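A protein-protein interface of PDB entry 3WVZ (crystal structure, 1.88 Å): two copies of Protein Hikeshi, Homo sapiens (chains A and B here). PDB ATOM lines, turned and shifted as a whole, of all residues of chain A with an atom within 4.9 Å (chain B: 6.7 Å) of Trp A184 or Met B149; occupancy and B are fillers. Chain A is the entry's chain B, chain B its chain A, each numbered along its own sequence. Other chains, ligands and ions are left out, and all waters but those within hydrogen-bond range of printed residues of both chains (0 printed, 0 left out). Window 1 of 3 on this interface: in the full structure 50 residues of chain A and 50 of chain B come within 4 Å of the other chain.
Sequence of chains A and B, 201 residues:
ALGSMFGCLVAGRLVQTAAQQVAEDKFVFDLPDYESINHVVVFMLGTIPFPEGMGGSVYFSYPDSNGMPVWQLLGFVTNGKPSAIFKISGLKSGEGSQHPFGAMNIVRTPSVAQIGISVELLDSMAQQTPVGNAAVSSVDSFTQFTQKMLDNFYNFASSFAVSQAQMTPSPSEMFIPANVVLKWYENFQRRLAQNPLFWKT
Phe A145 touches Thr B146 (CZ to CB, 3.6 Å).
Leu B150 touches Met A149 (CA to SD, 3.8 Å).
Phe B156 touches Val A180 (CE2 to O, 3.9 Å).
CB of Ala B157 touches CG2 of Val A180, 3.8 Å away.
CZ2 of Trp A184 touches O of Met B149, 3.9 Å away.
Trp A184 touches Phe B153 (NE1 to CA, 3.6 Å).
Trp A184 touches Phe B156.
CZ3 of Trp A199 touches CD of Gln B144 (3.8 Å).
Phe B145 touches Trp A199.
Trp A199 touches Lys B148 (O to CD, 3.2 Å).
The indole nitrogen of Trp A184 lies within hydrogen-bond range of the side-chain amide oxygen of Asn B152, 2.7 Å away.
Printed residues of chain B within 4 Å of Trp A199: Gln B144, Phe B145, Lys B148 and Met B149.
Printed residues of chain A within 4 Å of Gln B144: Trp A199.
Printed residues of chain A within 4 Å of Thr B146: Phe A145.
Gln B147 touches none of the printed residues of chain A.
The nearest printed residue of chain B that does not touch Trp A184 is Ala B157 (5.8 Å).
Of the 15 printed residues of chain A, 7 touch a printed residue of chain B.
Hydrophobic or aromatic side chains of chain A within 4 Å of the printed part of chain B: Phe A145, Met A149, Leu A150, Val A180, Trp A184, Phe A188 and Trp A199.
Along chain A the printed residues that touch a printed residue of chain B span positions 145 to 199.
Hydrophobic or aromatic side chains of chain B within 4 Å of the printed part of chain A: Phe B145, Met B149, Leu B150, Phe B153, Phe B156 and Ala B157.
Phe B145 touches its own counterpart, Phe A145.
Phe A145 touches Thr B146, but with the chains exchanged Thr A146 does not touch Phe B145 (4.2 Å).
Met A149 touches Leu B150, but with the chains exchanged Leu A150 does not touch Met B149 (7.5 Å).
4 positions are printed for both chains.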
ATOM      1  N   PHE A 145       2.600 -14.582  12.161  1.00  0.00           N
ATOM      2  CA  PHE A 145       1.265 -14.291  11.621  1.00  0.00           C
ATOM      3  C   PHE A 145       0.233 -15.254  12.189  1.00  0.00           C
ATOM      4  O   PHE A 145      -0.842 -14.838  12.617  1.00  0.00           O
ATOM      5  CB  PHE A 145       1.216 -14.368  10.095  1.00  0.00           C
ATOM      6  CG  PHE A 145      -0.188 -14.361   9.546  1.00  0.00           C
ATOM      7  CD1 PHE A 145      -0.886 -13.173   9.391  1.00  0.00           C
ATOM      8  CD2 PHE A 145      -0.817 -15.549   9.217  1.00  0.00           C
ATOM      9  CE1 PHE A 145      -2.192 -13.168   8.890  1.00  0.00           C
ATOM     10  CE2 PHE A 145      -2.121 -15.557   8.723  1.00  0.00           C
ATOM     11  CZ  PHE A 145      -2.811 -14.361   8.561  1.00  0.00           C
ATOM     12  N   THR A 146       0.570 -16.538  12.184  1.00  0.00           N
ATOM     13  CA  THR A 146      -0.344 -17.590  12.630  1.00  0.00           C
ATOM     14  C   THR A 146      -0.758 -17.381  14.082  1.00  0.00           C
ATOM     15  O   THR A 146      -1.941 -17.480  14.435  1.00  0.00           O
ATOM     16  CB  THR A 146       0.301 -18.983  12.458  1.00  0.00           C
ATOM     17  OG1 THR A 146       0.213 -19.383  11.083  1.00  0.00           O
ATOM     18  CG2 THR A 146      -0.390 -20.018  13.325  1.00  0.00           C
ATOM     19  N   MET A 149      -3.111 -14.458  14.162  1.00  0.00           N
ATOM     20  CA  MET A 149      -4.408 -14.839  13.604  1.00  0.00           C
ATOM     21  C   MET A 149      -5.242 -15.602  14.633  1.00  0.00           C
ATOM     22  O   MET A 149      -6.419 -15.298  14.856  1.00  0.00           O
ATOM     23  CB  MET A 149      -4.228 -15.693  12.349  1.00  0.00           C
ATOM     24  CG  MET A 149      -5.544 -16.111  11.705  1.00  0.00           C
ATOM     25  SD  MET A 149      -5.347 -17.240  10.317  1.00  0.00           S
ATOM     26  CE  MET A 149      -4.850 -18.751  11.150  1.00  0.00           C
ATOM     27  N   LEU A 150      -4.622 -16.593  15.265  1.00  0.00           N
ATOM     28  CA  LEU A 150      -5.301 -17.389  16.281  1.00  0.00           C
ATOM     29  C   LEU A 150      -5.628 -16.578  17.531  1.00  0.00           C
ATOM     30  O   LEU A 150      -6.661 -16.802  18.165  1.00  0.00           O
ATOM     31  CB  LEU A 150      -4.452 -18.604  16.647  1.00  0.00           C
ATOM     32  CG  LEU A 150      -4.284 -19.584  15.488  1.00  0.00           C
ATOM     33  CD1 LEU A 150      -3.288 -20.678  15.838  1.00  0.00           C
ATOM     34  CD2 LEU A 150      -5.630 -20.183  15.090  1.00  0.00           C
ATOM     35  N   VAL A 180      -9.923 -26.660  18.734  1.00  0.00           N
ATOM     36  CA  VAL A 180      -9.438 -26.664  17.349  1.00  0.00           C
ATOM     37  C   VAL A 180      -8.325 -25.634  17.156  1.00  0.00           C
ATOM     38  O   VAL A 180      -7.497 -25.775  16.256  1.00  0.00           O
ATOM     39  CB  VAL A 180     -10.558 -26.384  16.317  1.00  0.00           C
ATOM     40  CG1 VAL A 180     -11.634 -27.460  16.392  1.00  0.00           C
ATOM     41  CG2 VAL A 180     -11.142 -24.988  16.498  1.00  0.00           C
ATOM     42  N   VAL A 181      -8.312 -24.604  18.000  1.00  0.00           N
ATOM     43  CA  VAL A 181      -7.249 -23.602  17.985  1.00  0.00           C
ATOM     44  C   VAL A 181      -5.901 -24.268  18.226  1.00  0.00           C
ATOM     45  O   VAL A 181      -4.959 -24.104  17.449  1.00  0.00           O
ATOM     46  CB  VAL A 181      -7.475 -22.522  19.059  1.00  0.00           C
ATOM     47  CG1 VAL A 181      -6.240 -21.626  19.193  1.00  0.00           C
ATOM     48  CG2 VAL A 181      -8.708 -21.703  18.735  1.00  0.00           C
ATOM     49  N   LEU A 182      -5.833 -25.036  19.306  1.00  0.00           N
ATOM     50  CA  LEU A 182      -4.610 -25.729  19.682  1.00  0.00           C
ATOM     51  C   LEU A 182      -4.225 -26.765  18.632  1.00  0.00           C
ATOM     52  O   LEU A 182      -3.071 -26.837  18.211  1.00  0.00           O
ATOM     53  CB  LEU A 182      -4.778 -26.399  21.048  1.00  0.00           C
ATOM     54  CG  LEU A 182      -5.243 -25.492  22.186  1.00  0.00           C
ATOM     55  CD1 LEU A 182      -5.588 -26.311  23.419  1.00  0.00           C
ATOM     56  CD2 LEU A 182      -4.180 -24.451  22.507  1.00  0.00           C
ATOM     57  N   LYS A 183      -5.199 -27.559  18.201  1.00  0.00           N
ATOM     58  CA  LYS A 183      -4.920 -28.654  17.284  1.00  0.00           C
ATOM     59  C   LYS A 183      -4.429 -28.155  15.931  1.00  0.00           C
ATOM     60  O   LYS A 183      -3.519 -28.739  15.348  1.00  0.00           O
ATOM     61  CB  LYS A 183      -6.157 -29.545  17.114  1.00  0.00           C
ATOM     62  CG  LYS A 183      -6.521 -30.280  18.400  1.00  0.00           C
ATOM     63  CD  LYS A 183      -7.435 -31.467  18.155  1.00  0.00           C
ATOM     64  CE  LYS A 183      -8.766 -31.035  17.593  1.00  0.00           C
ATOM     65  NZ  LYS A 183      -9.746 -32.153  17.635  1.00  0.00           N
ATOM     66  N   TRP A 184      -5.011 -27.072  15.432  1.00  0.00           N
ATOM     67  CA  TRP A 184      -4.584 -26.575  14.134  1.00  0.00           C
ATOM     68  C   TRP A 184      -3.189 -25.981  14.232  1.00  0.00           C
ATOM     69  O   TRP A 184      -2.360 -26.172  13.343  1.00  0.00           O
ATOM     70  CB  TRP A 184      -5.552 -25.536  13.578  1.00  0.00           C
ATOM     71  CG  TRP A 184      -5.118 -25.070  12.229  1.00  0.00           C
ATOM     72  CD1 TRP A 184      -5.375 -25.670  11.037  1.00  0.00           C
ATOM     73  CD2 TRP A 184      -4.306 -23.928  11.941  1.00  0.00           C
ATOM     74  NE1 TRP A 184      -4.788 -24.960  10.014  1.00  0.00           N
ATOM     75  CE2 TRP A 184      -4.126 -23.884  10.544  1.00  0.00           C
ATOM     76  CE3 TRP A 184      -3.720 -22.931  12.729  1.00  0.00           C
ATOM     77  CZ2 TRP A 184      -3.383 -22.888   9.916  1.00  0.00           C
ATOM     78  CZ3 TRP A 184      -2.984 -21.936  12.103  1.00  0.00           C
ATOM     79  CH2 TRP A 184      -2.823 -21.924  10.710  1.00  0.00           C
ATOM     80  N   TYR A 185      -2.935 -25.258  15.320  1.00  0.00           N
ATOM     81  CA  TYR A 185      -1.625 -24.663  15.535  1.00  0.00           C
ATOM     82  C   TYR A 185      -0.551 -25.754  15.598  1.00  0.00           C
ATOM     83  O   TYR A 185       0.509 -25.619  14.993  1.00  0.00           O
ATOM     84  CB  TYR A 185      -1.619 -23.820  16.810  1.00  0.00           C
ATOM     85  CG  TYR A 185      -0.289 -23.153  17.073  1.00  0.00           C
ATOM     86  CD1 TYR A 185       0.189 -22.161  16.227  1.00  0.00           C
ATOM     87  CD2 TYR A 185       0.489 -23.521  18.163  1.00  0.00           C
ATOM     88  CE1 TYR A 185       1.409 -21.548  16.461  1.00  0.00           C
ATOM     89  CE2 TYR A 185       1.705 -22.912  18.407  1.00  0.00           C
ATOM     90  CZ  TYR A 185       2.162 -21.930  17.554  1.00  0.00           C
ATOM     91  OH  TYR A 185       3.374 -21.328  17.797  1.00  0.00           O
ATOM     92  N   GLU A 186      -0.841 -26.841  16.312  1.00  0.00           N
ATOM     93  CA  GLU A 186       0.105 -27.958  16.414  1.00  0.00           C
ATOM     94  C   GLU A 186       0.391 -28.577  15.046  1.00  0.00           C
ATOM     95  O   GLU A 186       1.532 -28.926  14.734  1.00  0.00           O
ATOM     96  CB  GLU A 186      -0.432 -29.027  17.369  1.00  0.00           C
ATOM     97  CG  GLU A 186      -0.535 -28.567  18.815  1.00  0.00           C
ATOM     98  CD  GLU A 186      -1.501 -29.413  19.628  1.00  0.00           C
ATOM     99  OE1 GLU A 186      -1.799 -30.549  19.205  1.00  0.00           O
ATOM    100  OE2 GLU A 186      -1.964 -28.938  20.687  1.00  0.00           O
ATOM    101  N   ASN A 187      -0.652 -28.711  14.236  1.00  0.00           N
ATOM    102  CA  ASN A 187      -0.508 -29.239  12.885  1.00  0.00           C
ATOM    103  C   ASN A 187       0.284 -28.295  11.985  1.00  0.00           C
ATOM    104  O   ASN A 187       1.123 -28.737  11.200  1.00  0.00           O
ATOM    105  CB  ASN A 187      -1.881 -29.519  12.277  1.00  0.00           C
ATOM    106  CG  ASN A 187      -2.474 -30.832  12.762  1.00  0.00           C
ATOM    107  OD1 ASN A 187      -2.311 -31.872  12.126  1.00  0.00           O
ATOM    108  ND2 ASN A 187      -3.164 -30.788  13.897  1.00  0.00           N
ATOM    109  N   PHE A 188       0.023 -26.996  12.111  1.00  0.00           N
ATOM    110  CA  PHE A 188       0.790 -25.988  11.386  1.00  0.00           C
ATOM    111  C   PHE A 188       2.279 -26.067  11.715  1.00  0.00           C
ATOM    112  O   PHE A 188       3.118 -26.092  10.814  1.00  0.00           O
ATOM    113  CB  PHE A 188       0.270 -24.583  11.697  1.00  0.00           C
ATOM    114  CG  PHE A 188       1.180 -23.479  11.224  1.00  0.00           C
ATOM    115  CD1 PHE A 188       1.134 -23.037   9.911  1.00  0.00           C
ATOM    116  CD2 PHE A 188       2.080 -22.881  12.095  1.00  0.00           C
ATOM    117  CE1 PHE A 188       1.973 -22.026   9.470  1.00  0.00           C
ATOM    118  CE2 PHE A 188       2.922 -21.871  11.660  1.00  0.00           C
ATOM    119  CZ  PHE A 188       2.866 -21.443  10.347  1.00  0.00           C
ATOM    120  N   PHE A 198       5.727 -25.198   2.508  1.00  0.00           N
ATOM    121  CA  PHE A 198       4.749 -26.246   2.202  1.00  0.00           C
ATOM    122  C   PHE A 198       3.485 -25.668   1.569  1.00  0.00           C
ATOM    123  O   PHE A 198       2.823 -26.319   0.759  1.00  0.00           O
ATOM    124  CB  PHE A 198       4.381 -27.032   3.469  1.00  0.00           C
ATOM    125  CG  PHE A 198       3.529 -26.258   4.448  1.00  0.00           C
ATOM    126  CD1 PHE A 198       2.140 -26.299   4.372  1.00  0.00           C
ATOM    127  CD2 PHE A 198       4.115 -25.493   5.442  1.00  0.00           C
ATOM    128  CE1 PHE A 198       1.356 -25.585   5.269  1.00  0.00           C
ATOM    129  CE2 PHE A 198       3.337 -24.779   6.343  1.00  0.00           C
ATOM    130  CZ  PHE A 198       1.954 -24.827   6.254  1.00  0.00           C
ATOM    131  N   TRP A 199       3.165 -24.437   1.955  1.00  0.00           N
ATOM    132  CA  TRP A 199       1.953 -23.750   1.525  1.00  0.00           C
ATOM    133  C   TRP A 199       2.072 -23.167   0.116  1.00  0.00           C
ATOM    134  O   TRP A 199       1.067 -22.938  -0.558  1.00  0.00           O
ATOM    135  CB  TRP A 199       1.635 -22.627   2.515  1.00  0.00           C
ATOM    136  CG  TRP A 199       2.812 -21.720   2.704  1.00  0.00           C
ATOM    137  CD1 TRP A 199       3.809 -21.850   3.628  1.00  0.00           C
ATOM    138  CD2 TRP A 199       3.140 -20.562   1.923  1.00  0.00           C
ATOM    139  NE1 TRP A 199       4.728 -20.837   3.481  1.00  0.00           N
ATOM    140  CE2 TRP A 199       4.339 -20.034   2.440  1.00  0.00           C
ATOM    141  CE3 TRP A 199       2.529 -19.918   0.843  1.00  0.00           C
ATOM    142  CZ2 TRP A 199       4.941 -18.895   1.912  1.00  0.00           C
ATOM    143  CZ3 TRP A 199       3.131 -18.790   0.319  1.00  0.00           C
ATOM    144  CH2 TRP A 199       4.323 -18.288   0.853  1.00  0.00           C
ATOM    145  N   GLN B 144       0.042 -14.439  -0.215  1.00  0.00           N
ATOM    146  CA  GLN B 144      -0.479 -15.761  -0.529  1.00  0.00           C
ATOM    147  C   GLN B 144      -0.523 -16.635   0.721  1.00  0.00           C
ATOM    148  O   GLN B 144      -1.489 -17.369   0.948  1.00  0.00           O
ATOM    149  CB  GLN B 144       0.376 -16.430  -1.611  1.00  0.00           C
ATOM    150  CG  GLN B 144      -0.003 -17.877  -1.899  1.00  0.00           C
ATOM    151  CD  GLN B 144       1.002 -18.584  -2.792  1.00  0.00           C
ATOM    152  OE1 GLN B 144       1.099 -19.812  -2.782  1.00  0.00           O
ATOM    153  NE2 GLN B 144       1.757 -17.813  -3.566  1.00  0.00           N
ATOM    154  N   PHE B 145       0.529 -16.546   1.530  1.00  0.00           N
ATOM    155  CA  PHE B 145       0.622 -17.318   2.761  1.00  0.00           C
ATOM    156  C   PHE B 145      -0.528 -17.021   3.725  1.00  0.00           C
ATOM    157  O   PHE B 145      -1.180 -17.939   4.227  1.00  0.00           O
ATOM    158  CB  PHE B 145       1.953 -17.048   3.464  1.00  0.00           C
ATOM    159  CG  PHE B 145       2.030 -17.622   4.848  1.00  0.00           C
ATOM    160  CD1 PHE B 145       2.244 -18.979   5.039  1.00  0.00           C
ATOM    161  CD2 PHE B 145       1.885 -16.807   5.964  1.00  0.00           C
ATOM    162  CE1 PHE B 145       2.317 -19.516   6.318  1.00  0.00           C
ATOM    163  CE2 PHE B 145       1.953 -17.336   7.245  1.00  0.00           C
ATOM    164  CZ  PHE B 145       2.168 -18.691   7.422  1.00  0.00           C
ATOM    165  N   THR B 146      -0.764 -15.737   3.987  1.00  0.00           N
ATOM    166  CA  THR B 146      -1.769 -15.332   4.968  1.00  0.00           C
ATOM    167  C   THR B 146      -3.169 -15.765   4.527  1.00  0.00           C
ATOM    168  O   THR B 146      -3.967 -16.241   5.339  1.00  0.00           O
ATOM    169  CB  THR B 146      -1.741 -13.803   5.210  1.00  0.00           C
ATOM    170  OG1 THR B 146      -1.989 -13.111   3.980  1.00  0.00           O
ATOM    171  CG2 THR B 146      -0.390 -13.378   5.751  1.00  0.00           C
ATOM    172  N   GLN B 147      -3.451 -15.617   3.237  1.00  0.00           N
ATOM    173  CA  GLN B 147      -4.736 -16.024   2.675  1.00  0.00           C
ATOM    174  C   GLN B 147      -4.940 -17.529   2.778  1.00  0.00           C
ATOM    175  O   GLN B 147      -6.033 -18.000   3.110  1.00  0.00           O
ATOM    176  CB  GLN B 147      -4.845 -15.588   1.213  1.00  0.00           C
ATOM    177  CG  GLN B 147      -4.940 -14.084   1.019  1.00  0.00           C
ATOM    178  CD  GLN B 147      -4.750 -13.668  -0.428  1.00  0.00           C
ATOM    179  OE1 GLN B 147      -4.076 -14.352  -1.199  1.00  0.00           O
ATOM    180  NE2 GLN B 147      -5.346 -12.544  -0.804  1.00  0.00           N
ATOM    181  N   LYS B 148      -3.888 -18.286   2.485  1.00  0.00           N
ATOM    182  CA  LYS B 148      -3.972 -19.738   2.557  1.00  0.00           C
ATOM    183  C   LYS B 148      -4.134 -20.223   3.993  1.00  0.00           C
ATOM    184  O   LYS B 148      -4.921 -21.133   4.250  1.00  0.00           O
ATOM    185  CB  LYS B 148      -2.741 -20.386   1.920  1.00  0.00           C
ATOM    186  CG  LYS B 148      -2.787 -20.402   0.404  1.00  0.00           C
ATOM    187  CD  LYS B 148      -1.601 -21.146  -0.182  1.00  0.00           C
ATOM    188  CE  LYS B 148      -1.685 -21.199  -1.700  1.00  0.00           C
ATOM    189  NZ  LYS B 148      -2.931 -21.866  -2.161  1.00  0.00           N
ATOM    190  N   MET B 149      -3.391 -19.632   4.925  1.00  0.00           N
ATOM    191  CA  MET B 149      -3.496 -20.060   6.319  1.00  0.00           C
ATOM    192  C   MET B 149      -4.883 -19.766   6.876  1.00  0.00           C
ATOM    193  O   MET B 149      -5.442 -20.572   7.621  1.00  0.00           O
ATOM    194  CB  MET B 149      -2.426 -19.396   7.180  1.00  0.00           C
ATOM    195  CG  MET B 149      -1.015 -19.884   6.884  1.00  0.00           C
ATOM    196  SD  MET B 149      -0.787 -21.679   6.994  1.00  0.00           S
ATOM    197  CE  MET B 149      -0.905 -22.158   5.273  1.00  0.00           C
ATOM    198  N   LEU B 150      -5.435 -18.614   6.510  1.00  0.00           N
ATOM    199  CA  LEU B 150      -6.777 -18.237   6.951  1.00  0.00           C
ATOM    200  C   LEU B 150      -7.818 -19.246   6.473  1.00  0.00           C
ATOM    201  O   LEU B 150      -8.633 -19.739   7.266  1.00  0.00           O
ATOM    202  CB  LEU B 150      -7.135 -16.834   6.451  1.00  0.00           C
ATOM    203  CG  LEU B 150      -8.506 -16.290   6.853  1.00  0.00           C
ATOM    204  CD1 LEU B 150      -8.663 -16.261   8.368  1.00  0.00           C
ATOM    205  CD2 LEU B 150      -8.720 -14.900   6.268  1.00  0.00           C
ATOM    206  N   ASP B 151      -7.785 -19.552   5.179  1.00  0.00           N
ATOM    207  CA  ASP B 151      -8.698 -20.534   4.606  1.00  0.00           C
ATOM    208  C   ASP B 151      -8.468 -21.921   5.196  1.00  0.00           C
ATOM    209  O   ASP B 151      -9.422 -22.659   5.450  1.00  0.00           O
ATOM    210  CB  ASP B 151      -8.550 -20.594   3.086  1.00  0.00           C
ATOM    211  CG  ASP B 151      -9.066 -19.350   2.393  1.00  0.00           C
ATOM    212  OD1 ASP B 151      -9.823 -18.576   3.020  1.00  0.00           O
ATOM    213  OD2 ASP B 151      -8.724 -19.156   1.210  1.00  0.00           O
ATOM    214  N   ASN B 152      -7.201 -22.273   5.406  1.00  0.00           N
ATOM    215  CA  ASN B 152      -6.849 -23.586   5.935  1.00  0.00           C
ATOM    216  C   ASN B 152      -7.389 -23.772   7.344  1.00  0.00           C
ATOM    217  O   ASN B 152      -7.987 -24.809   7.663  1.00  0.00           O
ATOM    218  CB  ASN B 152      -5.328 -23.782   5.924  1.00  0.00           C
ATOM    219  CG  ASN B 152      -4.920 -25.218   6.219  1.00  0.00           C
ATOM    220  OD1 ASN B 152      -4.918 -25.655   7.372  1.00  0.00           O
ATOM    221  ND2 ASN B 152      -4.565 -25.956   5.173  1.00  0.00           N
ATOM    222  N   PHE B 153      -7.172 -22.765   8.186  1.00  0.00           N
ATOM    223  CA  PHE B 153      -7.658 -22.802   9.560  1.00  0.00           C
ATOM    224  C   PHE B 153      -9.177 -22.900   9.605  1.00  0.00           C
ATOM    225  O   PHE B 153      -9.730 -23.737  10.323  1.00  0.00           O
ATOM    226  CB  PHE B 153      -7.198 -21.570  10.339  1.00  0.00           C
ATOM    227  CG  PHE B 153      -7.852 -21.433  11.684  1.00  0.00           C
ATOM    228  CD1 PHE B 153      -7.699 -22.418  12.649  1.00  0.00           C
ATOM    229  CD2 PHE B 153      -8.624 -20.320  11.982  1.00  0.00           C
ATOM    230  CE1 PHE B 153      -8.311 -22.294  13.886  1.00  0.00           C
ATOM    231  CE2 PHE B 153      -9.238 -20.192  13.214  1.00  0.00           C
ATOM    232  CZ  PHE B 153      -9.076 -21.182  14.171  1.00  0.00           C
ATOM    233  N   TYR B 154      -9.861 -22.061   8.837  1.00  0.00           N
ATOM    234  CA  TYR B 154     -11.318 -22.099   8.872  1.00  0.00           C
ATOM    235  C   TYR B 154     -11.875 -23.446   8.418  1.00  0.00           C
ATOM    236  O   TYR B 154     -12.805 -23.973   9.032  1.00  0.00           O
ATOM    237  CB  TYR B 154     -11.941 -21.003   8.021  1.00  0.00           C
ATOM    238  CG  TYR B 154     -13.443 -21.068   8.133  1.00  0.00           C
ATOM    239  CD1 TYR B 154     -14.086 -20.613   9.275  1.00  0.00           C
ATOM    240  CD2 TYR B 154     -14.213 -21.641   7.127  1.00  0.00           C
ATOM    241  CE1 TYR B 154     -15.463 -20.690   9.400  1.00  0.00           C
ATOM    242  CE2 TYR B 154     -15.591 -21.730   7.244  1.00  0.00           C
ATOM    243  CZ  TYR B 154     -16.206 -21.251   8.378  1.00  0.00           C
ATOM    244  OH  TYR B 154     -17.573 -21.334   8.501  1.00  0.00           O
ATOM    245  N   PHE B 156     -10.383 -26.328   8.522  1.00  0.00           N
ATOM    246  CA  PHE B 156     -10.036 -27.278   9.577  1.00  0.00           C
ATOM    247  C   PHE B 156     -10.995 -27.159  10.763  1.00  0.00           C
ATOM    248  O   PHE B 156     -11.557 -28.165  11.222  1.00  0.00           O
ATOM    249  CB  PHE B 156      -8.586 -27.049  10.022  1.00  0.00           C
ATOM    250  CG  PHE B 156      -8.122 -27.964  11.130  1.00  0.00           C
ATOM    251  CD1 PHE B 156      -7.480 -29.155  10.837  1.00  0.00           C
ATOM    252  CD2 PHE B 156      -8.300 -27.616  12.462  1.00  0.00           C
ATOM    253  CE1 PHE B 156      -7.033 -29.989  11.855  1.00  0.00           C
ATOM    254  CE2 PHE B 156      -7.858 -28.443  13.485  1.00  0.00           C
ATOM    255  CZ  PHE B 156      -7.223 -29.631  13.179  1.00  0.00           C
ATOM    256  N   ALA B 157     -11.173 -25.936  11.266  1.00  0.00           N
ATOM    257  CA  ALA B 157     -12.034 -25.716  12.430  1.00  0.00           C
ATOM    258  C   ALA B 157     -13.453 -26.193  12.139  1.00  0.00           C
ATOM    259  O   ALA B 157     -14.072 -26.877  12.959  1.00  0.00           O
ATOM    260  CB  ALA B 157     -12.037 -24.246  12.832  1.00  0.00           C
